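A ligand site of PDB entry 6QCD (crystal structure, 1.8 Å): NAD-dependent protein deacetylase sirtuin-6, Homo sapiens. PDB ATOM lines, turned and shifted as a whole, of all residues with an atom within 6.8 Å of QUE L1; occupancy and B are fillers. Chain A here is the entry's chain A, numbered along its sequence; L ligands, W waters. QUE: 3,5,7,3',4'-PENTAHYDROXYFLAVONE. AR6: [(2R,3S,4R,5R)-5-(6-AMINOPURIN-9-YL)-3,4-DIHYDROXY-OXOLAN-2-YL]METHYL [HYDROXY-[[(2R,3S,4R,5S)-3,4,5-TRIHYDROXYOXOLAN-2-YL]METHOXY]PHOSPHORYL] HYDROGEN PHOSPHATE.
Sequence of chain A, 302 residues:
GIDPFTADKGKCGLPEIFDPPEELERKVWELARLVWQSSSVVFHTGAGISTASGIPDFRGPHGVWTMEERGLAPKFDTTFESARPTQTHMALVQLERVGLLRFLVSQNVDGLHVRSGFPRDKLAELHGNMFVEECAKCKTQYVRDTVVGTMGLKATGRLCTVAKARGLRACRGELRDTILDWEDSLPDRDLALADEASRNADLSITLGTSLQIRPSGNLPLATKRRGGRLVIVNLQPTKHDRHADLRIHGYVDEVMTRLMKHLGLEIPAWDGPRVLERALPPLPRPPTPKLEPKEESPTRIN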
ATOM      1  N   ALA A  47     -24.250 -22.826 -11.620  1.00  0.00           N
ATOM      2  CA  ALA A  47     -24.480 -22.737 -10.155  1.00  0.00           C
ATOM      3  C   ALA A  47     -25.105 -24.022  -9.609  1.00  0.00           C
ATOM      4  O   ALA A  47     -24.866 -24.337  -8.381  1.00  0.00           O
ATOM      5  CB  ALA A  47     -25.331 -21.529  -9.831  1.00  0.00           C
ATOM      6  N   GLY A  48     -25.718 -24.837 -10.443  1.00  0.00           N
ATOM      7  CA  GLY A  48     -26.292 -26.143 -10.036  1.00  0.00           C
ATOM      8  C   GLY A  48     -25.247 -27.097  -9.454  1.00  0.00           C
ATOM      9  O   GLY A  48     -25.605 -27.978  -8.703  1.00  0.00           O
ATOM     10  N   SER A  50     -23.005 -26.450  -7.328  1.00  0.00           N
ATOM     11  CA  SER A  50     -22.534 -25.948  -6.023  1.00  0.00           C
ATOM     12  C   SER A  50     -23.656 -25.922  -4.978  1.00  0.00           C
ATOM     13  O   SER A  50     -23.401 -25.640  -3.799  1.00  0.00           O
ATOM     14  CB  SER A  50     -21.837 -24.644  -6.213  1.00  0.00           C
ATOM     15  OG  SER A  50     -20.621 -24.791  -6.975  1.00  0.00           O
ATOM     16  N   THR A  51     -24.895 -26.199  -5.400  1.00  0.00           N
ATOM     17  CA  THR A  51     -26.076 -26.245  -4.518  1.00  0.00           C
ATOM     18  C   THR A  51     -25.881 -27.301  -3.434  1.00  0.00           C
ATOM     19  O   THR A  51     -26.227 -27.026  -2.274  1.00  0.00           O
ATOM     20  CB  THR A  51     -27.380 -26.434  -5.305  1.00  0.00           C
ATOM     21  OG1 THR A  51     -27.328 -27.625  -6.064  1.00  0.00           O
ATOM     22  CG2 THR A  51     -27.755 -25.233  -6.155  1.00  0.00           C
ATOM     23  N   ILE A  55     -24.542 -23.479  -1.432  1.00  0.00           N
ATOM     24  CA  ILE A  55     -24.608 -22.181  -2.154  1.00  0.00           C
ATOM     25  C   ILE A  55     -25.782 -22.239  -3.108  1.00  0.00           C
ATOM     26  O   ILE A  55     -25.806 -23.171  -3.929  1.00  0.00           O
ATOM     27  CB  ILE A  55     -23.354 -21.969  -2.960  1.00  0.00           C
ATOM     28  CG1 ILE A  55     -22.139 -22.088  -2.046  1.00  0.00           C
ATOM     29  CG2 ILE A  55     -23.426 -20.643  -3.693  1.00  0.00           C
ATOM     30  CD1 ILE A  55     -20.873 -22.089  -2.812  1.00  0.00           C
ATOM     31  N   PRO A  56     -26.801 -21.382  -2.906  1.00  0.00           N
ATOM     32  CA  PRO A  56     -28.002 -21.454  -3.731  1.00  0.00           C
ATOM     33  C   PRO A  56     -27.671 -21.063  -5.170  1.00  0.00           C
ATOM     34  O   PRO A  56     -26.701 -20.312  -5.393  1.00  0.00           O
ATOM     35  CB  PRO A  56     -28.929 -20.435  -3.045  1.00  0.00           C
ATOM     36  CG  PRO A  56     -27.983 -19.384  -2.517  1.00  0.00           C
ATOM     37  CD  PRO A  56     -26.815 -20.222  -1.966  1.00  0.00           C
ATOM     38  N   ASP A  57     -28.423 -21.612  -6.123  1.00  0.00           N
ATOM     39  CA  ASP A  57     -28.248 -21.210  -7.542  1.00  0.00           C
ATOM     40  C   ASP A  57     -28.980 -19.860  -7.759  1.00  0.00           C
ATOM     41  O   ASP A  57     -29.376 -19.229  -6.752  1.00  0.00           O
ATOM     42  CB  ASP A  57     -28.646 -22.416  -8.411  1.00  0.00           C
ATOM     43  CG  ASP A  57     -30.127 -22.823  -8.308  1.00  0.00           C
ATOM     44  OD1 ASP A  57     -30.953 -22.042  -7.855  1.00  0.00           O
ATOM     45  OD2 ASP A  57     -30.429 -23.954  -8.681  1.00  0.00           O
ATOM     46  N   PHE A  58     -29.165 -19.455  -9.012  1.00  0.00           N
ATOM     47  CA  PHE A  58     -29.888 -18.198  -9.377  1.00  0.00           C
ATOM     48  C   PHE A  58     -31.343 -18.451  -9.759  1.00  0.00           C
ATOM     49  O   PHE A  58     -32.170 -17.609  -9.358  1.00  0.00           O
ATOM     50  CB  PHE A  58     -29.136 -17.508 -10.514  1.00  0.00           C
ATOM     51  CG  PHE A  58     -27.781 -17.064 -10.047  1.00  0.00           C
ATOM     52  CD1 PHE A  58     -27.658 -15.834  -9.441  1.00  0.00           C
ATOM     53  CD2 PHE A  58     -26.658 -17.887 -10.152  1.00  0.00           C
ATOM     54  CE1 PHE A  58     -26.446 -15.427  -8.905  1.00  0.00           C
ATOM     55  CE2 PHE A  58     -25.439 -17.434  -9.659  1.00  0.00           C
ATOM     56  CZ  PHE A  58     -25.346 -16.208  -9.031  1.00  0.00           C
ATOM     57  N   VAL A  64     -31.404 -17.400  -6.107  1.00  0.00           N
ATOM     58  CA  VAL A  64     -31.277 -15.978  -5.669  1.00  0.00           C
ATOM     59  C   VAL A  64     -32.363 -15.144  -6.385  1.00  0.00           C
ATOM     60  O   VAL A  64     -33.220 -14.485  -5.686  1.00  0.00           O
ATOM     61  CB  VAL A  64     -29.852 -15.482  -5.962  1.00  0.00           C
ATOM     62  CG1 VAL A  64     -29.734 -14.010  -5.668  1.00  0.00           C
ATOM     63  CG2 VAL A  64     -28.802 -16.256  -5.175  1.00  0.00           C
ATOM     64  N   PRO A  74     -32.602 -15.714  -0.743  1.00  0.00           N
ATOM     65  CA  PRO A  74     -31.918 -16.982  -0.850  1.00  0.00           C
ATOM     66  C   PRO A  74     -31.365 -17.362   0.535  1.00  0.00           C
ATOM     67  O   PRO A  74     -31.291 -16.495   1.386  1.00  0.00           O
ATOM     68  CB  PRO A  74     -30.863 -16.689  -1.918  1.00  0.00           C
ATOM     69  CG  PRO A  74     -30.499 -15.250  -1.659  1.00  0.00           C
ATOM     70  CD  PRO A  74     -31.864 -14.630  -1.436  1.00  0.00           C
ATOM     71  N   PHE A  76     -27.997 -19.240   2.260  1.00  0.00           N
ATOM     72  CA  PHE A  76     -26.635 -19.878   2.246  1.00  0.00           C
ATOM     73  C   PHE A  76     -26.447 -20.791   3.448  1.00  0.00           C
ATOM     74  O   PHE A  76     -26.645 -20.303   4.571  1.00  0.00           O
ATOM     75  CB  PHE A  76     -25.565 -18.809   2.210  1.00  0.00           C
ATOM     76  CG  PHE A  76     -25.425 -18.129   0.879  1.00  0.00           C
ATOM     77  CD1 PHE A  76     -26.344 -17.189   0.472  1.00  0.00           C
ATOM     78  CD2 PHE A  76     -24.329 -18.394   0.087  1.00  0.00           C
ATOM     79  CE1 PHE A  76     -26.163 -16.511  -0.711  1.00  0.00           C
ATOM     80  CE2 PHE A  76     -24.190 -17.749  -1.131  1.00  0.00           C
ATOM     81  CZ  PHE A  76     -25.098 -16.811  -1.510  1.00  0.00           C
ATOM     82  N   PHE A  80     -18.579 -18.620   1.479  1.00  0.00           N
ATOM     83  CA  PHE A  80     -17.756 -19.000   0.320  1.00  0.00           C
ATOM     84  C   PHE A  80     -16.457 -19.617   0.794  1.00  0.00           C
ATOM     85  O   PHE A  80     -15.918 -20.581   0.123  1.00  0.00           O
ATOM     86  CB  PHE A  80     -17.554 -17.778  -0.587  1.00  0.00           C
ATOM     87  CG  PHE A  80     -18.793 -17.396  -1.358  1.00  0.00           C
ATOM     88  CD1 PHE A  80     -19.285 -18.201  -2.372  1.00  0.00           C
ATOM     89  CD2 PHE A  80     -19.405 -16.193  -1.102  1.00  0.00           C
ATOM     90  CE1 PHE A  80     -20.379 -17.812  -3.131  1.00  0.00           C
ATOM     91  CE2 PHE A  80     -20.537 -15.810  -1.818  1.00  0.00           C
ATOM     92  CZ  PHE A  80     -21.021 -16.629  -2.825  1.00  0.00           C
ATOM     93  N   GLN A 107     -19.426 -20.678 -15.454  1.00  0.00           N
ATOM     94  CA  GLN A 107     -20.038 -19.370 -15.161  1.00  0.00           C
ATOM     95  C   GLN A 107     -19.946 -19.030 -13.683  1.00  0.00           C
ATOM     96  O   GLN A 107     -20.486 -18.008 -13.321  1.00  0.00           O
ATOM     97  CB  GLN A 107     -21.493 -19.451 -15.676  1.00  0.00           C
ATOM     98  CG  GLN A 107     -21.584 -19.574 -17.199  1.00  0.00           C
ATOM     99  CD  GLN A 107     -22.984 -19.896 -17.649  1.00  0.00           C
ATOM    100  OE1 GLN A 107     -23.865 -19.052 -17.621  1.00  0.00           O
ATOM    101  NE2 GLN A 107     -23.236 -21.136 -17.993  1.00  0.00           N
ATOM    102  N   ASN A 108     -19.388 -19.903 -12.839  1.00  0.00           N
ATOM    103  CA  ASN A 108     -19.501 -19.828 -11.375  1.00  0.00           C
ATOM    104  C   ASN A 108     -18.435 -18.849 -10.891  1.00  0.00           C
ATOM    105  O   ASN A 108     -17.259 -18.921 -11.393  1.00  0.00           O
ATOM    106  CB  ASN A 108     -19.383 -21.193 -10.684  1.00  0.00           C
ATOM    107  CG  ASN A 108     -20.558 -22.088 -11.014  1.00  0.00           C
ATOM    108  OD1 ASN A 108     -21.604 -21.585 -11.432  1.00  0.00           O
ATOM    109  ND2 ASN A 108     -20.364 -23.387 -10.866  1.00  0.00           N
ATOM    110  N   VAL A 109     -18.863 -17.944 -10.005  1.00  0.00           N
ATOM    111  CA  VAL A 109     -17.980 -16.980  -9.284  1.00  0.00           C
ATOM    112  C   VAL A 109     -17.550 -17.551  -7.899  1.00  0.00           C
ATOM    113  O   VAL A 109     -16.852 -16.854  -7.161  1.00  0.00           O
ATOM    114  CB  VAL A 109     -18.654 -15.599  -9.107  1.00  0.00           C
ATOM    115  CG1 VAL A 109     -18.971 -15.009 -10.449  1.00  0.00           C
ATOM    116  CG2 VAL A 109     -19.873 -15.651  -8.181  1.00  0.00           C
ATOM    117  N   ASP A 110     -18.038 -18.719  -7.512  1.00  0.00           N
ATOM    118  CA  ASP A 110     -17.880 -19.281  -6.142  1.00  0.00           C
ATOM    119  C   ASP A 110     -16.440 -19.732  -5.834  1.00  0.00           C
ATOM    120  O   ASP A 110     -16.166 -20.000  -4.664  1.00  0.00           O
ATOM    121  CB  ASP A 110     -18.911 -20.402  -5.927  1.00  0.00           C
ATOM    122  CG  ASP A 110     -18.797 -21.602  -6.825  1.00  0.00           C
ATOM    123  OD1 ASP A 110     -17.658 -21.951  -7.222  1.00  0.00           O
ATOM    124  OD2 ASP A 110     -19.855 -22.188  -7.187  1.00  0.00           O
ATOM    125  N   GLY A 111     -15.522 -19.745  -6.816  1.00  0.00           N
ATOM    126  CA  GLY A 111     -14.123 -20.102  -6.591  1.00  0.00           C
ATOM    127  C   GLY A 111     -13.868 -21.571  -6.249  1.00  0.00           C
ATOM    128  O   GLY A 111     -12.684 -21.950  -5.962  1.00  0.00           O
ATOM    129  N   MET A 130     -14.713 -14.931  -7.018  1.00  0.00           N
ATOM    130  CA  MET A 130     -14.886 -14.116  -5.792  1.00  0.00           C
ATOM    131  C   MET A 130     -13.523 -13.955  -5.108  1.00  0.00           C
ATOM    132  O   MET A 130     -13.354 -13.003  -4.390  1.00  0.00           O
ATOM    133  CB  MET A 130     -15.819 -14.760  -4.735  1.00  0.00           C
ATOM    134  CG  MET A 130     -17.316 -14.646  -5.005  1.00  0.00           C
ATOM    135  SD  MET A 130     -17.932 -12.930  -5.013  1.00  0.00           S
ATOM    136  CE  MET A 130     -17.776 -12.423  -3.290  1.00  0.00           C
ATOM    137  N   MET A 151     -17.120  -6.055  -5.917  1.00  0.00           N
ATOM    138  CA  MET A 151     -17.689  -6.648  -7.166  1.00  0.00           C
ATOM    139  C   MET A 151     -17.823  -5.515  -8.182  1.00  0.00           C
ATOM    140  O   MET A 151     -17.867  -4.365  -7.736  1.00  0.00           O
ATOM    141  CB  MET A 151     -19.037  -7.293  -6.893  1.00  0.00           C
ATOM    142  CG  MET A 151     -18.912  -8.434  -5.886  1.00  0.00           C
ATOM    143  SD  MET A 151     -20.457  -9.081  -5.166  1.00  0.00           S
ATOM    144  CE  MET A 151     -21.675  -8.525  -6.352  1.00  0.00           C
ATOM    145  N   ILE A 179     -15.251  -9.728 -10.579  1.00  0.00           N
ATOM    146  CA  ILE A 179     -16.710  -9.998 -10.667  1.00  0.00           C
ATOM    147  C   ILE A 179     -17.341  -9.028 -11.677  1.00  0.00           C
ATOM    148  O   ILE A 179     -17.464  -7.821 -11.388  1.00  0.00           O
ATOM    149  CB  ILE A 179     -17.387 -10.032  -9.302  1.00  0.00           C
ATOM    150  CG1 ILE A 179     -16.697 -11.022  -8.366  1.00  0.00           C
ATOM    151  CG2 ILE A 179     -18.881 -10.370  -9.444  1.00  0.00           C
ATOM    152  CD1 ILE A 179     -16.697 -12.451  -8.857  1.00  0.00           C
HETATM  153  C1  QUE L   1     -24.389 -10.583  -1.353  1.00  0.00           C
HETATM  154  C2  QUE L   1     -23.353 -10.867  -2.215  1.00  0.00           C
HETATM  155  C3  QUE L   1     -23.394 -12.018  -3.036  1.00  0.00           C
HETATM  156  C4  QUE L   1     -24.521 -12.828  -2.969  1.00  0.00           C
HETATM  157  C5  QUE L   1     -25.601 -12.560  -2.133  1.00  0.00           C
HETATM  158  C6  QUE L   1     -25.507 -11.445  -1.313  1.00  0.00           C
HETATM  159  C9  QUE L   1     -22.306 -12.368  -3.929  1.00  0.00           C
HETATM  160  C10 QUE L   1     -22.475 -13.569  -4.695  1.00  0.00           C
HETATM  161  C11 QUE L   1     -23.625 -14.307  -4.619  1.00  0.00           C
HETATM  162  C14 QUE L   1     -23.849 -15.582  -5.302  1.00  0.00           C
HETATM  163  C15 QUE L   1     -25.098 -16.184  -5.234  1.00  0.00           C
HETATM  164  C16 QUE L   1     -25.301 -17.467  -5.743  1.00  0.00           C
HETATM  165  C17 QUE L   1     -24.269 -18.136  -6.367  1.00  0.00           C
HETATM  166  C18 QUE L   1     -22.986 -17.577  -6.386  1.00  0.00           C
HETATM  167  C19 QUE L   1     -22.772 -16.318  -5.850  1.00  0.00           C
HETATM  168  O12 QUE L   1     -24.630 -13.944  -3.747  1.00  0.00           O
HETATM  169  O13 QUE L   1     -21.253 -11.708  -4.039  1.00  0.00           O
HETATM  170  O23 QUE L   1     -21.968 -18.280  -6.974  1.00  0.00           O
HETATM  171  O24 QUE L   1     -24.524 -19.339  -6.959  1.00  0.00           O
HETATM  172  O27 QUE L   1     -21.460 -13.881  -5.532  1.00  0.00           O
HETATM  173  O29 QUE L   1     -26.522 -11.134  -0.476  1.00  0.00           O
HETATM  174  O30 QUE L   1     -22.256 -10.085  -2.262  1.00  0.00           O
HETATM  175  N1  AR6 L   2     -28.197 -31.107  -9.798  1.00  0.00           N
HETATM  176  C2  AR6 L   2     -28.652 -30.785 -11.020  1.00  0.00           C
HETATM  177  N3  AR6 L   2     -29.134 -29.617 -11.466  1.00  0.00           N
HETATM  178  C4  AR6 L   2     -29.137 -28.691 -10.488  1.00  0.00           C
HETATM  179  C5  AR6 L   2     -28.765 -28.882  -9.174  1.00  0.00           C
HETATM  180  C6  AR6 L   2     -28.271 -30.167  -8.827  1.00  0.00           C
HETATM  181  N6  AR6 L   2     -27.835 -30.511  -7.614  1.00  0.00           N
HETATM  182  N7  AR6 L   2     -28.968 -27.724  -8.443  1.00  0.00           N
HETATM  183  C8  AR6 L   2     -29.402 -26.843  -9.331  1.00  0.00           C
HETATM  184  N9  AR6 L   2     -29.553 -27.379 -10.581  1.00  0.00           N
HETATM  185  PA  AR6 L   2     -28.996 -20.962 -12.937  1.00  0.00           P
HETATM  186  PB  AR6 L   2     -26.370 -20.436 -14.138  1.00  0.00           P
HETATM  187  C1' AR6 L   2     -29.942 -26.697 -11.750  1.00  0.00           C
HETATM  188  O1A AR6 L   2     -29.608 -20.259 -14.107  1.00  0.00           O
HETATM  189  O1B AR6 L   2     -25.040 -20.799 -13.553  1.00  0.00           O
HETATM  190  C1D AR6 L   2     -26.471 -15.328 -13.154  1.00  0.00           C
HETATM  191  O1D AR6 L   2     -26.881 -14.022 -13.407  1.00  0.00           O
HETATM  192  C2' AR6 L   2     -31.197 -25.831 -11.660  1.00  0.00           C
HETATM  193  O2' AR6 L   2     -32.384 -26.534 -11.969  1.00  0.00           O
HETATM  194  O2A AR6 L   2     -29.451 -20.858 -11.527  1.00  0.00           O
HETATM  195  O2B AR6 L   2     -26.790 -21.130 -15.365  1.00  0.00           O
HETATM  196  C2D AR6 L   2     -24.990 -15.361 -12.806  1.00  0.00           C
HETATM  197  O2D AR6 L   2     -24.288 -14.276 -13.403  1.00  0.00           O
HETATM  198  C3' AR6 L   2     -30.883 -24.681 -12.613  1.00  0.00           C
HETATM  199  O3' AR6 L   2     -31.620 -24.673 -13.822  1.00  0.00           O
HETATM  200  O3A AR6 L   2     -27.401 -20.657 -12.897  1.00  0.00           O
HETATM  201  C3D AR6 L   2     -24.603 -16.761 -13.276  1.00  0.00           C
HETATM  202  O3D AR6 L   2     -23.175 -16.928 -13.344  1.00  0.00           O
HETATM  203  C4' AR6 L   2     -29.361 -24.756 -12.872  1.00  0.00           C
HETATM  204  O4' AR6 L   2     -28.894 -25.801 -12.030  1.00  0.00           O
HETATM  205  C4D AR6 L   2     -25.368 -16.783 -14.611  1.00  0.00           C
HETATM  206  O4D AR6 L   2     -26.611 -16.091 -14.336  1.00  0.00           O
HETATM  207  C5' AR6 L   2     -28.568 -23.532 -12.547  1.00  0.00           C
HETATM  208  O5' AR6 L   2     -29.076 -22.476 -13.423  1.00  0.00           O
HETATM  209  C5D AR6 L   2     -25.699 -18.147 -15.156  1.00  0.00           C
HETATM  210  O5D AR6 L   2     -26.474 -18.849 -14.157  1.00  0.00           O
HETATM  211  O   HOH W   1     -21.731 -17.565 -10.006  1.00  0.00           O
HETATM  212  O   HOH W   2     -24.499 -22.436  -6.448  1.00  0.00           O
HETATM  213  O   HOH W   3     -24.532  -8.984  -4.408  1.00  0.00           O
HETATM  214  O   HOH W   4     -26.028 -11.975  -5.974  1.00  0.00           O
HETATM  215  O   HOH W   5     -22.262 -21.031  -7.446  1.00  0.00           O
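An oxygen (O30) of QUE L1 lies within hydrogen-bond range of the side-chain sulfur of Met 151.
The side-chain hydroxyl of Thr 51 is in hydrogen-bond range of a nitrogen (N7) of AR6 L2 (2.9 Å).
O of Pro 56 sits at hydrogen-bond distance from O24 of QUE L1 (2.9 Å).
O of Gln 107 is in hydrogen-bond range of O3D of AR6 L2, 2.9 Å away.
The backbone NH (N) of Phe 58 lies within hydrogen-bond range of an oxygen (O2A) of AR6 L2.
The side-chain sulfur of Met 130 sits at hydrogen-bond distance from an oxygen (O27) of QUE L1, 3.7 Å away.
The backbone NH of Ala 47 is in hydrogen-bond range of an oxygen (O1B) of AR6 L2.
Ala 47 touches QUE L1 (CB to O24, 3.7 Å).
Ile 55 touches QUE L1 (CG2 to O24, 3.7 Å).
CE2 of Phe 58 touches O24 of QUE L1, 3.4 Å away.
CG2 of Val 64 touches C15 of QUE L1, 3.7 Å away.
Phe 76 touches QUE L1.
Phe 80 touches QUE L1 (CZ to C19, 3.5 Å).
Val 109 touches QUE L1 (CG2 to O27, 3.6 Å).
Asp 110 touches QUE L1.
Hydrophobic or aromatic side chains within 4 Å of QUE L1: Ala 47, Ile 55, Phe 58, Val 64, Phe 76, Phe 80, Val 109, Met 130 and Met 151.
Water W5 bridges OD2 of Asp 110 (2.7 Å) and O23 of QUE L1 (2.8 Å).
Water W1 lies within hydrogen-bond range of N of Val 109 and O23 of QUE L1.
The backbone carbonyl oxygen (O) of Val 109 sits at hydrogen-bond distance from the backbone NH (N) of Met 130, at 2.9 Å.
The backbone NH of Ala 47 sits at hydrogen-bond distance from the side-chain amide oxygen of Asn 108, 2.9 Å away.
The side-chain carboxylate of Asp 110 lies within hydrogen-bond range of the side-chain hydroxyl of Ser 50 (2.7 Å).
The backbone NH of Val 64 lies within hydrogen-bond range of the backbone carbonyl oxygen of Phe 58.
N of Val 64 is in hydrogen-bond range of O of Asp 57 (2.8 Å).
N of Ile 55 is in hydrogen-bond range of O of Ser 50 (3.4 Å).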
